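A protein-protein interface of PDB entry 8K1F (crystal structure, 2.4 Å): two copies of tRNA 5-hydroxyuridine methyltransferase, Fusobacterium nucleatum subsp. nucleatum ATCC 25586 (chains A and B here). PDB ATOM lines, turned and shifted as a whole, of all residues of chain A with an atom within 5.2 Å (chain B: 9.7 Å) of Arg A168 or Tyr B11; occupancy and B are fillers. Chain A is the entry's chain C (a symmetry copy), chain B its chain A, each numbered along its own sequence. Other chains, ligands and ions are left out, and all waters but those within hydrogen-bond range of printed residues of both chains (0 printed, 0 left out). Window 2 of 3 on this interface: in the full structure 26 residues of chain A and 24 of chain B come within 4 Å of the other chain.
The side-chain carboxylate (OE2) of Glu B45 lies close to the backbone carbonyl oxygen (O) of Leu A201 (3.5 Å). The side-chain carboxylate (OD1) of Asp A187 is in salt-bridge range of the side-chain amino group (NZ) of Lys B15 (3.2 Å). The side-chain carboxylate (OD1) of Asp A187 lies within hydrogen-bond range of the side-chain hydroxyl (OH) of Tyr B11 (2.4 Å).
Among the printed residues, merely in contact across the chains: Leu A166 with Tyr B11, Arg A168 with Tyr B11, Val A190 with Tyr B11, Val A190 with Lys B15 and Leu A201 with Ile B12.
No position is printed for both chains.
Ile A165 touches none of the printed residues of chain B. Leu A166 touches one residue of chain B. No residue of chain B comes within 4 Å of Phe A167. Arg A168 touches just one residue of chain B: Tyr B11. No residue of chain B comes within 4 Å of Gly A169. Asp A187 touches two residues of chain B. Of the printed residues of chain B, Leu A201 touches Ile B12 and Glu B45. Tyr B11 touches just these residues of chain A: Leu A166, Arg A168, Asp A187 and Val A190. Of the printed residues of chain A, Ile B12 touches Leu A201 (3.9 Å). Of the printed residues of chain A, Glu B45 touches Leu A201 (3.5 Å). The nearest residue of chain A that does not touch Tyr B11 is Leu A201 (4.03 Å). The nearest printed residue of chain B that does not touch Val A190 is Tyr B19 (5.4 Å).
Printed residues of chain B that touch a printed residue of chain A: Tyr B11, Ile B12, Lys B15 and Glu B45. Hydrophobic or aromatic side chains of chain B that line the printed part of chain A: Tyr B11 and Ile B12. Of the 12 printed residues of chain A, 5 touch a printed residue of chain B. Hydrophobic or aromatic side chains of chain A that line the printed part of chain B: Leu A166, Val A190 and Leu A201. Among the printed residues, 8 pairs touch across the chains. Among the printed residues, Asp or Glu carboxylates within 4 Å of a Lys or Arg side-chain nitrogen of the other chain: Asp A187 with Lys B15 (3.2 Å).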
ATOM      1  N   ILE A 165      15.600  -6.111  12.528  1.00  0.00           N
ATOM      2  CA  ILE A 165      14.215  -6.448  12.112  1.00  0.00           C
ATOM      3  C   ILE A 165      13.981  -7.967  12.086  1.00  0.00           C
ATOM      4  O   ILE A 165      12.869  -8.351  12.102  1.00  0.00           O
ATOM      5  CB  ILE A 165      13.798  -5.708  10.827  1.00  0.00           C
ATOM      6  CG1 ILE A 165      12.280  -5.582  10.775  1.00  0.00           C
ATOM      7  CG2 ILE A 165      14.348  -6.360   9.579  1.00  0.00           C
ATOM      8  CD1 ILE A 165      11.766  -4.615   9.792  1.00  0.00           C
ATOM      9  N   LEU A 166      15.022  -8.783  12.026  1.00  0.00           N
ATOM     10  CA  LEU A 166      14.824 -10.246  12.059  1.00  0.00           C
ATOM     11  C   LEU A 166      15.236 -10.815  13.421  1.00  0.00           C
ATOM     12  O   LEU A 166      15.381 -11.976  13.521  1.00  0.00           O
ATOM     13  CB  LEU A 166      15.563 -10.893  10.888  1.00  0.00           C
ATOM     14  CG  LEU A 166      15.042 -10.492   9.516  1.00  0.00           C
ATOM     15  CD1 LEU A 166      15.875 -11.077   8.411  1.00  0.00           C
ATOM     16  CD2 LEU A 166      13.607 -10.861   9.314  1.00  0.00           C
ATOM     17  N   PHE A 167      15.270  -9.996  14.452  1.00  0.00           N
ATOM     18  CA  PHE A 167      15.766 -10.399  15.785  1.00  0.00           C
ATOM     19  C   PHE A 167      14.979 -11.530  16.472  1.00  0.00           C
ATOM     20  O   PHE A 167      13.778 -11.452  16.628  1.00  0.00           O
ATOM     21  CB  PHE A 167      15.820  -9.162  16.662  1.00  0.00           C
ATOM     22  CG  PHE A 167      16.676  -9.372  17.866  1.00  0.00           C
ATOM     23  CD1 PHE A 167      17.977  -9.776  17.723  1.00  0.00           C
ATOM     24  CD2 PHE A 167      16.150  -9.264  19.129  1.00  0.00           C
ATOM     25  CE1 PHE A 167      18.751 -10.021  18.831  1.00  0.00           C
ATOM     26  CE2 PHE A 167      16.930  -9.500  20.237  1.00  0.00           C
ATOM     27  CZ  PHE A 167      18.229  -9.873  20.084  1.00  0.00           C
ATOM     28  N   ARG A 168      15.670 -12.557  16.948  1.00  0.00           N
ATOM     29  CA  ARG A 168      14.938 -13.617  17.677  1.00  0.00           C
ATOM     30  C   ARG A 168      15.679 -14.019  18.943  1.00  0.00           C
ATOM     31  O   ARG A 168      15.417 -15.024  19.441  1.00  0.00           O
ATOM     32  CB  ARG A 168      14.770 -14.886  16.843  1.00  0.00           C
ATOM     33  CG  ARG A 168      14.140 -14.732  15.475  1.00  0.00           C
ATOM     34  CD  ARG A 168      12.725 -14.290  15.546  1.00  0.00           C
ATOM     35  NE  ARG A 168      11.952 -14.488  14.345  1.00  0.00           N
ATOM     36  CZ  ARG A 168      11.331 -13.530  13.697  1.00  0.00           C
ATOM     37  NH1 ARG A 168      11.457 -12.278  14.075  1.00  0.00           N
ATOM     38  NH2 ARG A 168      10.618 -13.819  12.640  1.00  0.00           N
ATOM     39  N   GLY A 169      16.602 -13.165  19.401  1.00  0.00           N
ATOM     40  CA  GLY A 169      17.394 -13.444  20.615  1.00  0.00           C
ATOM     41  C   GLY A 169      16.710 -12.932  21.871  1.00  0.00           C
ATOM     42  O   GLY A 169      17.085 -11.842  22.345  1.00  0.00           O
ATOM     43  N   TYR A 170      15.739 -13.692  22.389  1.00  0.00           N
ATOM     44  CA  TYR A 170      14.997 -13.304  23.618  1.00  0.00           C
ATOM     45  C   TYR A 170      14.786 -14.543  24.496  1.00  0.00           C
ATOM     46  O   TYR A 170      14.590 -15.644  23.943  1.00  0.00           O
ATOM     47  CB  TYR A 170      13.654 -12.664  23.256  1.00  0.00           C
ATOM     48  CG  TYR A 170      13.752 -11.372  22.483  1.00  0.00           C
ATOM     49  CD1 TYR A 170      14.281 -10.229  23.060  1.00  0.00           C
ATOM     50  CD2 TYR A 170      13.314 -11.290  21.172  1.00  0.00           C
ATOM     51  CE1 TYR A 170      14.375  -9.041  22.357  1.00  0.00           C
ATOM     52  CE2 TYR A 170      13.400 -10.108  20.454  1.00  0.00           C
ATOM     53  CZ  TYR A 170      13.932  -8.979  21.048  1.00  0.00           C
ATOM     54  OH  TYR A 170      14.020  -7.810  20.348  1.00  0.00           O
ATOM     55  N   PHE A 179       7.656 -14.348  24.368  1.00  0.00           N
ATOM     56  CA  PHE A 179       8.504 -14.465  23.184  1.00  0.00           C
ATOM     57  C   PHE A 179       7.664 -14.503  21.911  1.00  0.00           C
ATOM     58  O   PHE A 179       7.939 -13.779  20.948  1.00  0.00           O
ATOM     59  CB  PHE A 179       9.367 -15.719  23.312  1.00  0.00           C
ATOM     60  CG  PHE A 179      10.365 -15.929  22.190  1.00  0.00           C
ATOM     61  CD1 PHE A 179       9.953 -16.367  20.935  1.00  0.00           C
ATOM     62  CD2 PHE A 179      11.720 -15.767  22.421  1.00  0.00           C
ATOM     63  CE1 PHE A 179      10.869 -16.606  19.928  1.00  0.00           C
ATOM     64  CE2 PHE A 179      12.633 -16.008  21.433  1.00  0.00           C
ATOM     65  CZ  PHE A 179      12.207 -16.428  20.172  1.00  0.00           C
ATOM     66  N   VAL A 183       7.712 -11.652  18.756  1.00  0.00           N
ATOM     67  CA  VAL A 183       8.034 -12.016  17.383  1.00  0.00           C
ATOM     68  C   VAL A 183       6.829 -11.801  16.470  1.00  0.00           C
ATOM     69  O   VAL A 183       6.978 -11.376  15.323  1.00  0.00           O
ATOM     70  CB  VAL A 183       8.547 -13.467  17.334  1.00  0.00           C
ATOM     71  CG1 VAL A 183       8.433 -14.020  15.932  1.00  0.00           C
ATOM     72  CG2 VAL A 183       9.990 -13.550  17.831  1.00  0.00           C
ATOM     73  N   LEU A 186       6.792  -8.215  15.503  1.00  0.00           N
ATOM     74  CA  LEU A 186       7.822  -7.978  14.497  1.00  0.00           C
ATOM     75  C   LEU A 186       7.346  -8.437  13.120  1.00  0.00           C
ATOM     76  O   LEU A 186       7.351  -7.661  12.159  1.00  0.00           O
ATOM     77  CB  LEU A 186       9.118  -8.688  14.899  1.00  0.00           C
ATOM     78  CG  LEU A 186      10.399  -7.890  14.698  1.00  0.00           C
ATOM     79  CD1 LEU A 186      10.313  -6.573  15.423  1.00  0.00           C
ATOM     80  CD2 LEU A 186      11.607  -8.660  15.182  1.00  0.00           C
ATOM     81  N   ASP A 187       6.886  -9.690  13.029  1.00  0.00           N
ATOM     82  CA  ASP A 187       6.439 -10.261  11.762  1.00  0.00           C
ATOM     83  C   ASP A 187       5.290  -9.459  11.170  1.00  0.00           C
ATOM     84  O   ASP A 187       5.225  -9.267   9.949  1.00  0.00           O
ATOM     85  CB  ASP A 187       6.023 -11.719  11.968  1.00  0.00           C
ATOM     86  CG  ASP A 187       5.749 -12.452  10.655  1.00  0.00           C
ATOM     87  OD1 ASP A 187       6.715 -12.694   9.895  1.00  0.00           O
ATOM     88  OD2 ASP A 187       4.572 -12.802  10.387  1.00  0.00           O
ATOM     89  N   VAL A 190       6.886  -6.380   9.610  1.00  0.00           N
ATOM     90  CA  VAL A 190       7.425  -6.693   8.293  1.00  0.00           C
ATOM     91  C   VAL A 190       6.302  -6.714   7.261  1.00  0.00           C
ATOM     92  O   VAL A 190       6.397  -6.076   6.209  1.00  0.00           O
ATOM     93  CB  VAL A 190       8.191  -8.028   8.319  1.00  0.00           C
ATOM     94  CG1 VAL A 190       8.456  -8.515   6.896  1.00  0.00           C
ATOM     95  CG2 VAL A 190       9.478  -7.866   9.059  1.00  0.00           C
ATOM     96  N   LEU A 201      13.968  -6.102   2.612  1.00  0.00           N
ATOM     97  CA  LEU A 201      14.397  -6.940   3.714  1.00  0.00           C
ATOM     98  C   LEU A 201      15.761  -7.488   3.358  1.00  0.00           C
ATOM     99  O   LEU A 201      15.908  -8.116   2.303  1.00  0.00           O
ATOM    100  CB  LEU A 201      13.422  -8.093   3.932  1.00  0.00           C
ATOM    101  CG  LEU A 201      12.566  -8.091   5.173  1.00  0.00           C
ATOM    102  CD1 LEU A 201      12.132  -9.524   5.414  1.00  0.00           C
ATOM    103  CD2 LEU A 201      13.350  -7.554   6.331  1.00  0.00           C
ATOM    104  N   TYR B  11      12.841 -17.095   5.364  1.00  0.00           N
ATOM    105  CA  TYR B  11      11.894 -16.105   5.877  1.00  0.00           C
ATOM    106  C   TYR B  11      11.645 -14.980   4.869  1.00  0.00           C
ATOM    107  O   TYR B  11      10.502 -14.596   4.606  1.00  0.00           O
ATOM    108  CB  TYR B  11      12.396 -15.516   7.201  1.00  0.00           C
ATOM    109  CG  TYR B  11      11.451 -14.491   7.819  1.00  0.00           C
ATOM    110  CD1 TYR B  11      11.553 -13.138   7.504  1.00  0.00           C
ATOM    111  CD2 TYR B  11      10.460 -14.873   8.718  1.00  0.00           C
ATOM    112  CE1 TYR B  11      10.693 -12.196   8.062  1.00  0.00           C
ATOM    113  CE2 TYR B  11       9.594 -13.933   9.287  1.00  0.00           C
ATOM    114  CZ  TYR B  11       9.716 -12.597   8.943  1.00  0.00           C
ATOM    115  OH  TYR B  11       8.867 -11.653   9.481  1.00  0.00           O
ATOM    116  N   ILE B  12      12.735 -14.453   4.312  1.00  0.00           N
ATOM    117  CA  ILE B  12      12.635 -13.339   3.376  1.00  0.00           C
ATOM    118  C   ILE B  12      11.991 -13.780   2.062  1.00  0.00           C
ATOM    119  O   ILE B  12      11.116 -13.096   1.517  1.00  0.00           O
ATOM    120  CB  ILE B  12      14.023 -12.725   3.152  1.00  0.00           C
ATOM    121  CG1 ILE B  12      14.647 -12.364   4.506  1.00  0.00           C
ATOM    122  CG2 ILE B  12      13.911 -11.523   2.238  1.00  0.00           C
ATOM    123  CD1 ILE B  12      16.109 -11.920   4.417  1.00  0.00           C
ATOM    124  N   SER B  13      12.413 -14.928   1.528  1.00  0.00           N
ATOM    125  CA  SER B  13      11.784 -15.438   0.310  1.00  0.00           C
ATOM    126  C   SER B  13      10.295 -15.718   0.530  1.00  0.00           C
ATOM    127  O   SER B  13       9.472 -15.501  -0.373  1.00  0.00           O
ATOM    128  CB  SER B  13      12.509 -16.697  -0.174  1.00  0.00           C
ATOM    129  N   SER B  14       9.928 -16.207   1.719  1.00  0.00           N
ATOM    130  CA  SER B  14       8.509 -16.341   2.034  1.00  0.00           C
ATOM    131  C   SER B  14       7.808 -14.986   1.944  1.00  0.00           C
ATOM    132  O   SER B  14       6.682 -14.885   1.439  1.00  0.00           O
ATOM    133  CB  SER B  14       8.334 -16.964   3.420  1.00  0.00           C
ATOM    134  N   LYS B  15       8.475 -13.923   2.390  1.00  0.00           N
ATOM    135  CA  LYS B  15       7.861 -12.608   2.273  1.00  0.00           C
ATOM    136  C   LYS B  15       7.829 -12.140   0.820  1.00  0.00           C
ATOM    137  O   LYS B  15       6.831 -11.562   0.374  1.00  0.00           O
ATOM    138  CB  LYS B  15       8.594 -11.606   3.166  1.00  0.00           C
ATOM    139  CG  LYS B  15       8.466 -11.880   4.656  1.00  0.00           C
ATOM    140  CD  LYS B  15       7.013 -11.900   5.116  1.00  0.00           C
ATOM    141  CE  LYS B  15       6.910 -12.159   6.615  1.00  0.00           C
ATOM    142  NZ  LYS B  15       5.486 -12.260   7.025  1.00  0.00           N
ATOM    143  N   ILE B  16       8.896 -12.389   0.057  1.00  0.00           N
ATOM    144  CA  ILE B  16       8.935 -11.889  -1.317  1.00  0.00           C
ATOM    145  C   ILE B  16       7.906 -12.604  -2.186  1.00  0.00           C
ATOM    146  O   ILE B  16       7.203 -11.977  -2.992  1.00  0.00           O
ATOM    147  CB  ILE B  16      10.347 -12.031  -1.904  1.00  0.00           C
ATOM    148  CG1 ILE B  16      11.317 -11.077  -1.202  1.00  0.00           C
ATOM    149  CG2 ILE B  16      10.313 -11.758  -3.392  1.00  0.00           C
ATOM    150  CD1 ILE B  16      12.774 -11.525  -1.276  1.00  0.00           C
ATOM    151  N   ASP B  17       7.824 -13.926  -2.062  1.00  0.00           N
ATOM    152  CA  ASP B  17       6.764 -14.659  -2.746  1.00  0.00           C
ATOM    153  C   ASP B  17       5.389 -14.183  -2.283  1.00  0.00           C
ATOM    154  O   ASP B  17       4.454 -14.084  -3.087  1.00  0.00           O
ATOM    155  CB  ASP B  17       6.956 -16.162  -2.516  1.00  0.00           C
ATOM    156  CG  ASP B  17       7.958 -16.783  -3.505  1.00  0.00           C
ATOM    157  OD1 ASP B  17       8.181 -16.181  -4.581  1.00  0.00           O
ATOM    158  OD2 ASP B  17       8.532 -17.863  -3.212  1.00  0.00           O
ATOM    159  N   LYS B  18       5.279 -13.894  -0.982  1.00  0.00           N
ATOM    160  CA  LYS B  18       4.003 -13.425  -0.378  1.00  0.00           C
ATOM    161  C   LYS B  18       3.623 -12.068  -0.982  1.00  0.00           C
ATOM    162  O   LYS B  18       2.456 -11.909  -1.390  1.00  0.00           O
ATOM    163  CB  LYS B  18       4.138 -13.330   1.145  1.00  0.00           C
ATOM    164  N   TYR B  19       4.578 -11.133  -1.030  1.00  0.00           N
ATOM    165  CA  TYR B  19       4.326  -9.778  -1.590  1.00  0.00           C
ATOM    166  C   TYR B  19       5.207  -9.561  -2.826  1.00  0.00           C
ATOM    167  O   TYR B  19       4.672  -9.540  -3.952  1.00  0.00           O
ATOM    168  CB  TYR B  19       4.575  -8.704  -0.528  1.00  0.00           C
ATOM    169  CG  TYR B  19       3.792  -8.885   0.747  1.00  0.00           C
ATOM    170  CD1 TYR B  19       2.439  -8.599   0.802  1.00  0.00           C
ATOM    171  CD2 TYR B  19       4.403  -9.342   1.904  1.00  0.00           C
ATOM    172  CE1 TYR B  19       1.711  -8.762   1.970  1.00  0.00           C
ATOM    173  CE2 TYR B  19       3.692  -9.511   3.080  1.00  0.00           C
ATOM    174  CZ  TYR B  19       2.339  -9.220   3.113  1.00  0.00           C
ATOM    175  OH  TYR B  19       1.631  -9.383   4.269  1.00  0.00           O
ATOM    176  N   LYS B  44      15.573 -14.543  -5.661  1.00  0.00           N
ATOM    177  CA  LYS B  44      14.482 -13.646  -5.306  1.00  0.00           C
ATOM    178  C   LYS B  44      15.001 -12.463  -4.503  1.00  0.00           C
ATOM    179  O   LYS B  44      14.494 -11.344  -4.635  1.00  0.00           O
ATOM    180  CB  LYS B  44      13.410 -14.398  -4.515  1.00  0.00           C
ATOM    181  N   GLU B  45      16.022 -12.709  -3.709  1.00  0.00           N
ATOM    182  CA  GLU B  45      16.550 -11.668  -2.814  1.00  0.00           C
ATOM    183  C   GLU B  45      17.357 -10.660  -3.617  1.00  0.00           C
ATOM    184  O   GLU B  45      17.222  -9.496  -3.366  1.00  0.00           O
ATOM    185  CB  GLU B  45      17.347 -12.316  -1.701  1.00  0.00           C
ATOM    186  CG  GLU B  45      16.546 -12.590  -0.463  1.00  0.00           C
ATOM    187  CD  GLU B  45      17.349 -12.270   0.780  1.00  0.00           C
ATOM    188  OE1 GLU B  45      18.189 -13.094   1.162  1.00  0.00           O
ATOM    189  OE2 GLU B  45      17.171 -11.173   1.322  1.00  0.00           O
